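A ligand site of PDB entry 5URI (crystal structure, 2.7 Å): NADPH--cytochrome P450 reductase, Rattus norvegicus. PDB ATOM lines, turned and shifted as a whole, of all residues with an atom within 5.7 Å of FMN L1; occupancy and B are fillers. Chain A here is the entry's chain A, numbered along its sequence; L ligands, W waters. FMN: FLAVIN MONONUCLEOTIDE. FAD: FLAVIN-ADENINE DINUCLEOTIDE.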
ATOM      1  N   GLY A  29      24.684 -18.666  -0.517  1.00  0.00           N
ATOM      2  CA  GLY A  29      25.309 -17.567  -1.233  1.00  0.00           C
ATOM      3  C   GLY A  29      24.580 -16.360  -0.697  1.00  0.00           C
ATOM      4  O   GLY A  29      23.609 -15.871  -1.283  1.00  0.00           O
ATOM      5  N   SER A  30      25.043 -15.880   0.457  1.00  0.00           N
ATOM      6  CA  SER A  30      24.401 -14.749   1.119  1.00  0.00           C
ATOM      7  C   SER A  30      25.338 -13.582   1.361  1.00  0.00           C
ATOM      8  O   SER A  30      26.538 -13.749   1.573  1.00  0.00           O
ATOM      9  CB  SER A  30      23.811 -15.213   2.451  1.00  0.00           C
ATOM     10  OG  SER A  30      23.071 -14.192   3.057  1.00  0.00           O
ATOM     11  N   GLN A  31      24.771 -12.389   1.364  1.00  0.00           N
ATOM     12  CA  GLN A  31      25.542 -11.176   1.605  1.00  0.00           C
ATOM     13  C   GLN A  31      24.866 -10.399   2.723  1.00  0.00           C
ATOM     14  O   GLN A  31      25.524  -9.810   3.573  1.00  0.00           O
ATOM     15  CB  GLN A  31      25.616 -10.344   0.337  1.00  0.00           C
ATOM     16  CG  GLN A  31      26.785  -9.416   0.271  1.00  0.00           C
ATOM     17  CD  GLN A  31      27.079  -8.994  -1.153  1.00  0.00           C
ATOM     18  OE1 GLN A  31      27.523  -9.801  -1.968  1.00  0.00           O
ATOM     19  NE2 GLN A  31      26.801  -7.726  -1.460  1.00  0.00           N
ATOM     20  N   THR A  32      23.533 -10.428   2.727  1.00  0.00           N
ATOM     21  CA  THR A  32      22.731  -9.739   3.729  1.00  0.00           C
ATOM     22  C   THR A  32      22.170 -10.732   4.740  1.00  0.00           C
ATOM     23  O   THR A  32      21.311 -10.405   5.557  1.00  0.00           O
ATOM     24  CB  THR A  32      21.584  -8.980   3.064  1.00  0.00           C
ATOM     25  OG1 THR A  32      22.114  -8.147   2.031  1.00  0.00           O
ATOM     26  CG2 THR A  32      20.868  -8.110   4.074  1.00  0.00           C
ATOM     27  N   GLY A  33      22.669 -11.963   4.683  1.00  0.00           N
ATOM     28  CA  GLY A  33      22.233 -12.990   5.620  1.00  0.00           C
ATOM     29  C   GLY A  33      20.970 -13.784   5.340  1.00  0.00           C
ATOM     30  O   GLY A  33      20.699 -14.761   6.054  1.00  0.00           O
ATOM     31  N   THR A  34      20.212 -13.413   4.321  1.00  0.00           N
ATOM     32  CA  THR A  34      18.982 -14.149   4.043  1.00  0.00           C
ATOM     33  C   THR A  34      19.241 -15.580   3.598  1.00  0.00           C
ATOM     34  O   THR A  34      18.726 -16.521   4.218  1.00  0.00           O
ATOM     35  CB  THR A  34      18.131 -13.443   2.964  1.00  0.00           C
ATOM     36  OG1 THR A  34      18.079 -12.039   3.246  1.00  0.00           O
ATOM     37  CG2 THR A  34      16.696 -13.999   2.991  1.00  0.00           C
ATOM     38  N   ALA A  35      20.017 -15.765   2.538  1.00  0.00           N
ATOM     39  CA  ALA A  35      20.326 -17.089   2.001  1.00  0.00           C
ATOM     40  C   ALA A  35      20.788 -18.007   3.111  1.00  0.00           C
ATOM     41  O   ALA A  35      20.344 -19.158   3.220  1.00  0.00           O
ATOM     42  CB  ALA A  35      21.404 -16.988   0.931  1.00  0.00           C
ATOM     43  N   GLU A  36      21.689 -17.496   3.940  1.00  0.00           N
ATOM     44  CA  GLU A  36      22.204 -18.262   5.049  1.00  0.00           C
ATOM     45  C   GLU A  36      21.059 -18.712   5.942  1.00  0.00           C
ATOM     46  O   GLU A  36      21.004 -19.852   6.378  1.00  0.00           O
ATOM     47  CB  GLU A  36      23.174 -17.399   5.842  1.00  0.00           C
ATOM     48  CG  GLU A  36      23.971 -18.132   6.880  1.00  0.00           C
ATOM     49  CD  GLU A  36      24.653 -17.167   7.809  1.00  0.00           C
ATOM     50  OE1 GLU A  36      25.358 -16.261   7.321  1.00  0.00           O
ATOM     51  OE2 GLU A  36      24.476 -17.310   9.034  1.00  0.00           O
ATOM     52  N   ALA A  82      21.828 -16.137  -3.667  1.00  0.00           N
ATOM     53  CA  ALA A  82      21.233 -14.845  -3.976  1.00  0.00           C
ATOM     54  C   ALA A  82      22.086 -14.224  -5.071  1.00  0.00           C
ATOM     55  O   ALA A  82      23.246 -14.608  -5.237  1.00  0.00           O
ATOM     56  CB  ALA A  82      21.210 -13.954  -2.749  1.00  0.00           C
ATOM     57  N   THR A  83      21.517 -13.279  -5.797  1.00  0.00           N
ATOM     58  CA  THR A  83      22.223 -12.606  -6.874  1.00  0.00           C
ATOM     59  C   THR A  83      22.482 -11.142  -6.523  1.00  0.00           C
ATOM     60  O   THR A  83      21.714 -10.544  -5.768  1.00  0.00           O
ATOM     61  CB  THR A  83      21.395 -12.650  -8.167  1.00  0.00           C
ATOM     62  OG1 THR A  83      21.159 -14.000  -8.539  1.00  0.00           O
ATOM     63  CG2 THR A  83      22.137 -11.954  -9.288  1.00  0.00           C
ATOM     64  N   TYR A  84      23.560 -10.588  -7.062  1.00  0.00           N
ATOM     65  CA  TYR A  84      23.913  -9.179  -6.831  1.00  0.00           C
ATOM     66  C   TYR A  84      24.411  -8.490  -8.098  1.00  0.00           C
ATOM     67  O   TYR A  84      25.175  -9.066  -8.866  1.00  0.00           O
ATOM     68  CB  TYR A  84      24.940  -9.033  -5.705  1.00  0.00           C
ATOM     69  CG  TYR A  84      24.307  -9.116  -4.339  1.00  0.00           C
ATOM     70  CD1 TYR A  84      23.873 -10.341  -3.821  1.00  0.00           C
ATOM     71  CD2 TYR A  84      24.057  -7.961  -3.600  1.00  0.00           C
ATOM     72  CE1 TYR A  84      23.213 -10.414  -2.597  1.00  0.00           C
ATOM     73  CE2 TYR A  84      23.389  -8.029  -2.382  1.00  0.00           C
ATOM     74  CZ  TYR A  84      22.976  -9.249  -1.885  1.00  0.00           C
ATOM     75  OH  TYR A  84      22.331  -9.310  -0.672  1.00  0.00           O
ATOM     76  N   GLY A  85      23.952  -7.254  -8.287  1.00  0.00           N
ATOM     77  CA  GLY A  85      24.316  -6.439  -9.441  1.00  0.00           C
ATOM     78  C   GLY A  85      24.824  -7.124 -10.698  1.00  0.00           C
ATOM     79  O   GLY A  85      25.916  -7.701 -10.698  1.00  0.00           O
ATOM     80  N   GLU A  86      24.048  -7.048 -11.771  1.00  0.00           N
ATOM     81  CA  GLU A  86      24.432  -7.646 -13.062  1.00  0.00           C
ATOM     82  C   GLU A  86      24.465  -9.168 -12.984  1.00  0.00           C
ATOM     83  O   GLU A  86      25.337  -9.807 -13.577  1.00  0.00           O
ATOM     84  CB  GLU A  86      25.806  -7.130 -13.500  1.00  0.00           C
ATOM     85  CG  GLU A  86      25.965  -5.615 -13.413  1.00  0.00           C
ATOM     86  CD  GLU A  86      27.415  -5.171 -13.491  1.00  0.00           C
ATOM     87  OE1 GLU A  86      27.686  -3.979 -13.232  1.00  0.00           O
ATOM     88  OE2 GLU A  86      28.286  -6.010 -13.809  1.00  0.00           O
ATOM     89  N   GLY A  87      23.502  -9.739 -12.269  1.00  0.00           N
ATOM     90  CA  GLY A  87      23.429 -11.178 -12.129  1.00  0.00           C
ATOM     91  C   GLY A  87      24.722 -11.799 -11.616  1.00  0.00           C
ATOM     92  O   GLY A  87      25.126 -12.867 -12.067  1.00  0.00           O
ATOM     93  N   ASP A  88      25.372 -11.125 -10.672  1.00  0.00           N
ATOM     94  CA  ASP A  88      26.612 -11.628 -10.110  1.00  0.00           C
ATOM     95  C   ASP A  88      26.375 -12.391  -8.821  1.00  0.00           C
ATOM     96  O   ASP A  88      25.353 -12.205  -8.150  1.00  0.00           O
ATOM     97  CB  ASP A  88      27.600 -10.479  -9.856  1.00  0.00           C
ATOM     98  CG  ASP A  88      28.265  -9.982 -11.129  1.00  0.00           C
ATOM     99  OD1 ASP A  88      28.895 -10.796 -11.838  1.00  0.00           O
ATOM    100  OD2 ASP A  88      28.157  -8.768 -11.407  1.00  0.00           O
ATOM    101  N   THR A  90      27.162 -13.623  -4.868  1.00  0.00           N
ATOM    102  CA  THR A  90      27.451 -12.837  -3.689  1.00  0.00           C
ATOM    103  C   THR A  90      28.964 -12.992  -3.512  1.00  0.00           C
ATOM    104  O   THR A  90      29.545 -13.981  -3.953  1.00  0.00           O
ATOM    105  CB  THR A  90      26.695 -13.377  -2.465  1.00  0.00           C
ATOM    106  OG1 THR A  90      27.059 -14.739  -2.225  1.00  0.00           O
ATOM    107  CG2 THR A  90      25.202 -13.296  -2.696  1.00  0.00           C
ATOM    108  N   LEU A 117      17.498 -16.768  -4.439  1.00  0.00           N
ATOM    109  CA  LEU A 117      16.964 -15.573  -3.816  1.00  0.00           C
ATOM    110  C   LEU A 117      17.253 -14.422  -4.772  1.00  0.00           C
ATOM    111  O   LEU A 117      18.412 -14.113  -5.040  1.00  0.00           O
ATOM    112  CB  LEU A 117      17.644 -15.289  -2.464  1.00  0.00           C
ATOM    113  CG  LEU A 117      17.398 -16.200  -1.256  1.00  0.00           C
ATOM    114  CD1 LEU A 117      18.287 -17.430  -1.323  1.00  0.00           C
ATOM    115  CD2 LEU A 117      17.691 -15.420   0.018  1.00  0.00           C
ATOM    116  N   GLY A 118      16.197 -13.809  -5.297  1.00  0.00           N
ATOM    117  CA  GLY A 118      16.389 -12.704  -6.213  1.00  0.00           C
ATOM    118  C   GLY A 118      15.365 -11.588  -6.021  1.00  0.00           C
ATOM    119  O   GLY A 118      14.749 -11.466  -4.970  1.00  0.00           O
ATOM    120  N   ASN A 119      15.194 -10.774  -7.061  1.00  0.00           N
ATOM    121  CA  ASN A 119      14.250  -9.681  -6.993  1.00  0.00           C
ATOM    122  C   ASN A 119      13.861  -9.238  -8.400  1.00  0.00           C
ATOM    123  O   ASN A 119      14.634  -8.568  -9.083  1.00  0.00           O
ATOM    124  CB  ASN A 119      14.861  -8.513  -6.228  1.00  0.00           C
ATOM    125  CG  ASN A 119      13.845  -7.432  -5.942  1.00  0.00           C
ATOM    126  OD1 ASN A 119      13.103  -7.015  -6.842  1.00  0.00           O
ATOM    127  ND2 ASN A 119      13.807  -6.974  -4.704  1.00  0.00           N
ATOM    128  N   LYS A 120      12.660  -9.622  -8.830  1.00  0.00           N
ATOM    129  CA  LYS A 120      12.173  -9.327 -10.167  1.00  0.00           C
ATOM    130  C   LYS A 120      12.454  -7.956 -10.759  1.00  0.00           C
ATOM    131  O   LYS A 120      12.481  -7.813 -11.980  1.00  0.00           O
ATOM    132  CB  LYS A 120      10.671  -9.621 -10.262  1.00  0.00           C
ATOM    133  CG  LYS A 120      10.306 -11.095 -10.209  1.00  0.00           C
ATOM    134  CD  LYS A 120       8.913 -11.313 -10.823  1.00  0.00           C
ATOM    135  CE  LYS A 120       8.448 -12.760 -10.743  1.00  0.00           C
ATOM    136  NZ  LYS A 120       8.177 -13.191  -9.343  1.00  0.00           N
ATOM    137  N   TYR A 122      15.280  -6.324 -10.761  1.00  0.00           N
ATOM    138  CA  TYR A 122      16.604  -6.277 -11.374  1.00  0.00           C
ATOM    139  C   TYR A 122      16.682  -6.928 -12.754  1.00  0.00           C
ATOM    140  O   TYR A 122      15.858  -7.774 -13.094  1.00  0.00           O
ATOM    141  CB  TYR A 122      17.651  -6.904 -10.443  1.00  0.00           C
ATOM    142  CG  TYR A 122      17.818  -6.134  -9.147  1.00  0.00           C
ATOM    143  CD1 TYR A 122      16.943  -6.338  -8.071  1.00  0.00           C
ATOM    144  CD2 TYR A 122      18.843  -5.186  -8.998  1.00  0.00           C
ATOM    145  CE1 TYR A 122      17.070  -5.620  -6.888  1.00  0.00           C
ATOM    146  CE2 TYR A 122      18.986  -4.464  -7.813  1.00  0.00           C
ATOM    147  CZ  TYR A 122      18.088  -4.680  -6.761  1.00  0.00           C
ATOM    148  OH  TYR A 122      18.218  -3.969  -5.590  1.00  0.00           O
ATOM    149  N   GLU A 123      17.664  -6.497 -13.538  1.00  0.00           N
ATOM    150  CA  GLU A 123      17.859  -6.996 -14.904  1.00  0.00           C
ATOM    151  C   GLU A 123      18.018  -8.514 -14.943  1.00  0.00           C
ATOM    152  O   GLU A 123      17.216  -9.214 -15.567  1.00  0.00           O
ATOM    153  CB  GLU A 123      19.080  -6.326 -15.533  1.00  0.00           C
ATOM    154  CG  GLU A 123      18.979  -6.123 -17.054  1.00  0.00           C
ATOM    155  CD  GLU A 123      17.923  -5.090 -17.431  1.00  0.00           C
ATOM    156  OE1 GLU A 123      17.996  -3.941 -16.936  1.00  0.00           O
ATOM    157  OE2 GLU A 123      17.002  -5.416 -18.223  1.00  0.00           O
ATOM    158  N   HIS A 124      19.054  -9.010 -14.289  1.00  0.00           N
ATOM    159  CA  HIS A 124      19.299 -10.443 -14.262  1.00  0.00           C
ATOM    160  C   HIS A 124      18.700 -11.083 -13.004  1.00  0.00           C
ATOM    161  O   HIS A 124      19.398 -11.316 -12.007  1.00  0.00           O
ATOM    162  CB  HIS A 124      20.811 -10.712 -14.352  1.00  0.00           C
ATOM    163  CG  HIS A 124      21.473  -9.963 -15.464  1.00  0.00           C
ATOM    164  ND1 HIS A 124      21.721  -8.607 -15.402  1.00  0.00           N
ATOM    165  CD2 HIS A 124      21.915 -10.373 -16.676  1.00  0.00           C
ATOM    166  CE1 HIS A 124      22.286  -8.216 -16.529  1.00  0.00           C
ATOM    167  NE2 HIS A 124      22.421  -9.267 -17.318  1.00  0.00           N
ATOM    168  N   PHE A 125      17.402 -11.342 -13.074  1.00  0.00           N
ATOM    169  CA  PHE A 125      16.625 -11.944 -12.003  1.00  0.00           C
ATOM    170  C   PHE A 125      17.126 -13.340 -11.638  1.00  0.00           C
ATOM    171  O   PHE A 125      17.119 -14.250 -12.479  1.00  0.00           O
ATOM    172  CB  PHE A 125      15.164 -12.000 -12.425  1.00  0.00           C
ATOM    173  CG  PHE A 125      14.281 -12.743 -11.477  1.00  0.00           C
ATOM    174  CD1 PHE A 125      14.135 -12.326 -10.154  1.00  0.00           C
ATOM    175  CD2 PHE A 125      13.578 -13.871 -11.909  1.00  0.00           C
ATOM    176  CE1 PHE A 125      13.313 -13.017  -9.276  1.00  0.00           C
ATOM    177  CE2 PHE A 125      12.760 -14.576 -11.031  1.00  0.00           C
ATOM    178  CZ  PHE A 125      12.624 -14.150  -9.711  1.00  0.00           C
ATOM    179  N   ASN A 126      17.553 -13.518 -10.394  1.00  0.00           N
ATOM    180  CA  ASN A 126      18.052 -14.813  -9.927  1.00  0.00           C
ATOM    181  C   ASN A 126      19.038 -15.442 -10.890  1.00  0.00           C
ATOM    182  O   ASN A 126      18.992 -16.652 -11.134  1.00  0.00           O
ATOM    183  CB  ASN A 126      16.880 -15.779  -9.710  1.00  0.00           C
ATOM    184  CG  ASN A 126      16.327 -15.696  -8.305  1.00  0.00           C
ATOM    185  OD1 ASN A 126      17.061 -15.847  -7.325  1.00  0.00           O
ATOM    186  ND2 ASN A 126      15.013 -15.488  -8.191  1.00  0.00           N
ATOM    187  N   ALA A 127      19.952 -14.651 -11.438  1.00  0.00           N
ATOM    188  CA  ALA A 127      20.919 -15.191 -12.371  1.00  0.00           C
ATOM    189  C   ALA A 127      21.800 -16.235 -11.705  1.00  0.00           C
ATOM    190  O   ALA A 127      22.080 -17.295 -12.289  1.00  0.00           O
ATOM    191  CB  ALA A 127      21.767 -14.074 -12.943  1.00  0.00           C
ATOM    192  N   ASP A 152      12.083 -11.329  -3.911  1.00  0.00           N
ATOM    193  CA  ASP A 152      12.073 -10.390  -2.796  1.00  0.00           C
ATOM    194  C   ASP A 152      11.189  -9.176  -3.078  1.00  0.00           C
ATOM    195  O   ASP A 152      10.944  -8.365  -2.182  1.00  0.00           O
ATOM    196  CB  ASP A 152      13.492  -9.922  -2.453  1.00  0.00           C
ATOM    197  CG  ASP A 152      13.577  -9.246  -1.087  1.00  0.00           C
ATOM    198  OD1 ASP A 152      12.900  -9.698  -0.151  1.00  0.00           O
ATOM    199  OD2 ASP A 152      14.332  -8.261  -0.951  1.00  0.00           O
ATOM    200  N   LEU A 156       9.615 -12.952  -0.573  1.00  0.00           N
ATOM    201  CA  LEU A 156      10.567 -14.050  -0.637  1.00  0.00           C
ATOM    202  C   LEU A 156      10.271 -15.131   0.396  1.00  0.00           C
ATOM    203  O   LEU A 156      10.309 -16.313   0.084  1.00  0.00           O
ATOM    204  CB  LEU A 156      11.997 -13.520  -0.472  1.00  0.00           C
ATOM    205  CG  LEU A 156      13.150 -14.533  -0.490  1.00  0.00           C
ATOM    206  CD1 LEU A 156      13.154 -15.341  -1.781  1.00  0.00           C
ATOM    207  CD2 LEU A 156      14.459 -13.777  -0.325  1.00  0.00           C
ATOM    208  N   VAL A 620      20.615   1.048  -7.961  1.00  0.00           N
ATOM    209  CA  VAL A 620      19.311   1.202  -7.326  1.00  0.00           C
ATOM    210  C   VAL A 620      19.276   0.307  -6.106  1.00  0.00           C
ATOM    211  O   VAL A 620      19.921  -0.737  -6.062  1.00  0.00           O
ATOM    212  CB  VAL A 620      18.160   0.814  -8.265  1.00  0.00           C
ATOM    213  CG1 VAL A 620      18.119   1.762  -9.459  1.00  0.00           C
ATOM    214  CG2 VAL A 620      18.328  -0.626  -8.736  1.00  0.00           C
HETATM  215  N1  FMN L   1      18.360  -9.807  -7.293  1.00  0.00           N
HETATM  216  C2  FMN L   1      18.388 -10.318  -8.538  1.00  0.00           C
HETATM  217  O2  FMN L   1      17.591 -11.194  -8.889  1.00  0.00           O
HETATM  218  N3  FMN L   1      19.344  -9.820  -9.396  1.00  0.00           N
HETATM  219  C4  FMN L   1      20.296  -8.825  -9.127  1.00  0.00           C
HETATM  220  O4  FMN L   1      21.044  -8.545 -10.053  1.00  0.00           O
HETATM  221  C4A FMN L   1      20.279  -8.268  -7.821  1.00  0.00           C
HETATM  222  N5  FMN L   1      21.225  -7.267  -7.515  1.00  0.00           N
HETATM  223  C5A FMN L   1      21.133  -6.765  -6.208  1.00  0.00           C
HETATM  224  C6  FMN L   1      22.076  -5.722  -5.868  1.00  0.00           C
HETATM  225  C7  FMN L   1      22.089  -5.128  -4.582  1.00  0.00           C
HETATM  226  C7M FMN L   1      23.159  -4.031  -4.362  1.00  0.00           C
HETATM  227  C8  FMN L   1      21.111  -5.561  -3.526  1.00  0.00           C
HETATM  228  C8M FMN L   1      21.024  -5.064  -2.256  1.00  0.00           C
HETATM  229  C9  FMN L   1      20.202  -6.559  -3.841  1.00  0.00           C
HETATM  230  C9A FMN L   1      20.174  -7.193  -5.175  1.00  0.00           C
HETATM  231  N10 FMN L   1      19.226  -8.258  -5.578  1.00  0.00           N
HETATM  232  C10 FMN L   1      19.281  -8.820  -6.945  1.00  0.00           C
HETATM  233  C1' FMN L   1      18.246  -8.756  -4.619  1.00  0.00           C
HETATM  234  C2' FMN L   1      18.793  -9.898  -3.714  1.00  0.00           C
HETATM  235  O2' FMN L   1      19.196 -11.028  -4.583  1.00  0.00           O
HETATM  236  C3' FMN L   1      17.730 -10.358  -2.739  1.00  0.00           C
HETATM  237  O3' FMN L   1      17.399  -9.203  -1.922  1.00  0.00           O
HETATM  238  C4' FMN L   1      18.310 -11.521  -1.864  1.00  0.00           C
HETATM  239  O4' FMN L   1      17.153 -11.843  -1.033  1.00  0.00           O
HETATM  240  C5' FMN L   1      19.396 -11.098  -0.894  1.00  0.00           C
HETATM  241  O5' FMN L   1      19.926 -12.228  -0.122  1.00  0.00           O
HETATM  242  P   FMN L   1      21.043 -12.156   0.999  1.00  0.00           P
HETATM  243  O1P FMN L   1      20.516 -11.402   2.173  1.00  0.00           O
HETATM  244  O2P FMN L   1      22.319 -11.646   0.246  1.00  0.00           O
HETATM  245  O3P FMN L   1      21.168 -13.702   1.407  1.00  0.00           O
HETATM  246  PA  FAD L   2      15.812   0.014   8.293  1.00  0.00           P
HETATM  247  O1A FAD L   2      15.661  -0.359   9.718  1.00  0.00           O
HETATM  248  O2A FAD L   2      16.755  -0.744   7.452  1.00  0.00           O
HETATM  249  O5B FAD L   2      14.363  -0.036   7.602  1.00  0.00           O
HETATM  250  C5B FAD L   2      14.275  -0.130   6.175  1.00  0.00           C
HETATM  251  C4B FAD L   2      12.924  -0.770   5.825  1.00  0.00           C
HETATM  252  O4B FAD L   2      11.857   0.063   6.294  1.00  0.00           O
HETATM  253  C3B FAD L   2      12.713  -0.770   4.326  1.00  0.00           C
HETATM  254  O3B FAD L   2      13.438  -1.875   3.769  1.00  0.00           O
HETATM  255  C2B FAD L   2      11.230  -1.082   4.312  1.00  0.00           C
HETATM  256  O2B FAD L   2      11.027  -2.495   4.438  1.00  0.00           O
HETATM  257  C1B FAD L   2      10.708  -0.357   5.551  1.00  0.00           C
HETATM  258  N9A FAD L   2       9.985   0.890   5.202  1.00  0.00           N
HETATM  259  C8A FAD L   2      10.608   2.175   4.821  1.00  0.00           C
HETATM  260  N7A FAD L   2       9.412   3.026   4.685  1.00  0.00           N
HETATM  261  C5A FAD L   2       8.330   2.278   4.907  1.00  0.00           C
HETATM  262  C6A FAD L   2       7.048   2.641   4.883  1.00  0.00           C
HETATM  263  N6A FAD L   2       6.814   3.953   4.865  1.00  0.00           N
HETATM  264  N1A FAD L   2       6.055   1.762   5.073  1.00  0.00           N
HETATM  265  C2A FAD L   2       6.375   0.426   5.321  1.00  0.00           C
HETATM  266  N3A FAD L   2       7.730   0.081   5.347  1.00  0.00           N
HETATM  267  C4A FAD L   2       8.666   1.011   5.131  1.00  0.00           C
HETATM  268  N1  FAD L   2      20.089   5.089   1.281  1.00  0.00           N
HETATM  269  C2  FAD L   2      20.373   6.461   1.310  1.00  0.00           C
HETATM  270  O2  FAD L   2      19.582   7.245   1.832  1.00  0.00           O
HETATM  271  N3  FAD L   2      21.501   6.948   0.639  1.00  0.00           N
HETATM  272  C4  FAD L   2      22.342   6.070  -0.049  1.00  0.00           C
HETATM  273  O4  FAD L   2      23.332   6.508  -0.623  1.00  0.00           O
HETATM  274  C4X FAD L   2      22.055   4.711  -0.079  1.00  0.00           C
HETATM  275  N5  FAD L   2      22.773   3.890  -0.860  1.00  0.00           N
HETATM  276  C5X FAD L   2      22.495   2.585  -0.882  1.00  0.00           C
HETATM  277  C6  FAD L   2      23.270   1.727  -1.664  1.00  0.00           C
HETATM  278  C7  FAD L   2      23.017   0.362  -1.664  1.00  0.00           C
HETATM  279  C7M FAD L   2      23.795  -0.480  -2.453  1.00  0.00           C
HETATM  280  C8  FAD L   2      21.992  -0.160  -0.884  1.00  0.00           C
HETATM  281  C8M FAD L   2      21.770  -1.532  -0.833  1.00  0.00           C
HETATM  282  C9  FAD L   2      21.217   0.698  -0.103  1.00  0.00           C
HETATM  283  C9A FAD L   2      21.474   2.064  -0.085  1.00  0.00           C
HETATM  284  N10 FAD L   2      20.749   2.898   0.680  1.00  0.00           N
HETATM  285  C10 FAD L   2      20.930   4.217   0.581  1.00  0.00           C
HETATM  286  C1' FAD L   2      19.660   2.374   1.551  1.00  0.00           C
HETATM  287  C2' FAD L   2      20.211   1.971   2.920  1.00  0.00           C
HETATM  288  O2' FAD L   2      21.104   0.866   2.763  1.00  0.00           O
HETATM  289  C3' FAD L   2      19.084   1.583   3.883  1.00  0.00           C
HETATM  290  O3' FAD L   2      18.168   0.710   3.215  1.00  0.00           O
HETATM  291  C4' FAD L   2      18.340   2.837   4.350  1.00  0.00           C
HETATM  292  O4' FAD L   2      19.281   3.805   4.818  1.00  0.00           O
HETATM  293  C5' FAD L   2      17.361   2.476   5.474  1.00  0.00           C
HETATM  294  O5' FAD L   2      18.054   1.798   6.515  1.00  0.00           O
HETATM  295  P   FAD L   2      17.708   2.039   8.068  1.00  0.00           P
HETATM  296  O1P FAD L   2      17.772   3.500   8.356  1.00  0.00           O
HETATM  297  O2P FAD L   2      18.530   1.117   8.885  1.00  0.00           O
HETATM  298  O3P FAD L   2      16.173   1.574   8.202  1.00  0.00           O
HETATM  299  O   HOH W   1      20.970  -7.538 -12.699  1.00  0.00           O
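The side-chain amide oxygen (OD1) of Asn 126 lies within hydrogen-bond range of the backbone NH (N) of Gly 118. The side-chain hydroxyl (OG) of Ser 30 sits at hydrogen-bond distance from the backbone NH (N) of Gly 33, 2.8 Å away. The side-chain amide oxygen (OD1) of Asn 126 sits close to the backbone NH (N) of Leu 117 (3.1 Å). The side-chain hydroxyl (OG) of Ser 30 sits at hydrogen-bond distance from the backbone NH (N) of Thr 34 (3.2 Å). The backbone carbonyl oxygen (O) of Gly 29 is in hydrogen-bond range of the backbone NH (N) of Ala 82 (3.0 Å). O of Leu 117 sits at hydrogen-bond distance from N of Thr 83 (3.3 Å). The side-chain hydroxyl (OH) of Tyr 84 lies within hydrogen-bond range of the side-chain hydroxyl (OG1) of Thr 32, 3.0 Å away. OG1 of Thr 83 is in hydrogen-bond range of N of Ala 127 (3.2 Å).
Ala 82 touches FMN L1. Glu 86 touches FMN L1 (N to O4, 3.8 Å). Gly 87 touches FMN L1 (N to O4, 3.5 Å). Gly 118 touches FMN L1. Tyr 122 touches FMN L1 (CD2 to N5, 3.5 Å). Phe 125 touches FMN L1. CD2 of Leu 156 touches O4' of FMN L1, 3.4 Å away. 21 residues have an atom within 4 Å of FMN L1: Ser 30, Gln 31, Thr 32, Gly 33, Thr 34, Ala 35, Ala 82, Thr 83, Tyr 84, Gly 85, Glu 86, Gly 87, Leu 117, Gly 118, Asn 119, Tyr 122, His 124, Phe 125, Asn 126, Asp 152 and Leu 156. The nearest printed residue that does not touch FMN L1 is Gly 29 (4.2 Å).
An oxygen (O3') of FMN L1 sits at hydrogen-bond distance from the side-chain carboxylate of Asp 152. An oxygen (O3P) of FMN L1 sits at hydrogen-bond distance from the backbone NH (N) of Ala 35 (2.6 Å). O2 of FMN L1 sits at hydrogen-bond distance from N of Asn 119, at 3.0 Å. O2 of FMN L1 is in hydrogen-bond range of N of Asn 126 (2.8 Å). The backbone NH of Gln 31 is in hydrogen-bond range of an oxygen (O2P) of FMN L1 (2.8 Å). The side-chain hydroxyl (OH) of Tyr 84 sits at hydrogen-bond distance from an oxygen (O2P) of FMN L1 (2.5 Å). A nitrogen (N3) of FMN L1 sits at hydrogen-bond distance from the backbone carbonyl oxygen (O) of His 124 (3.0 Å). The backbone carbonyl oxygen (O) of Leu 117 lies within hydrogen-bond range of an oxygen (O2') of FMN L1 (3.2 Å). An oxygen (O1P) of FMN L1 is in hydrogen-bond range of the backbone NH (N) of Gly 33, at 3.4 Å. The backbone NH (N) of Thr 34 sits at hydrogen-bond distance from an oxygen (O1P) of FMN L1 (3.0 Å). N of Gly 85 sits at hydrogen-bond distance from N5 of FMN L1, at 2.8 Å. The backbone NH (N) of Thr 83 is in hydrogen-bond range of an oxygen (O2') of FMN L1, 3.5 Å away. O2' of FMN L1 sits at hydrogen-bond distance from O of Thr 83. The backbone NH of Thr 32 lies within hydrogen-bond range of an oxygen (O2P) of FMN L1, 3.0 Å away. The side-chain hydroxyl (OG) of Ser 30 is in hydrogen-bond range of an oxygen (O3P) of FMN L1 (2.6 Å). OG1 of Thr 34 sits at hydrogen-bond distance from O1P of FMN L1 (2.7 Å).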
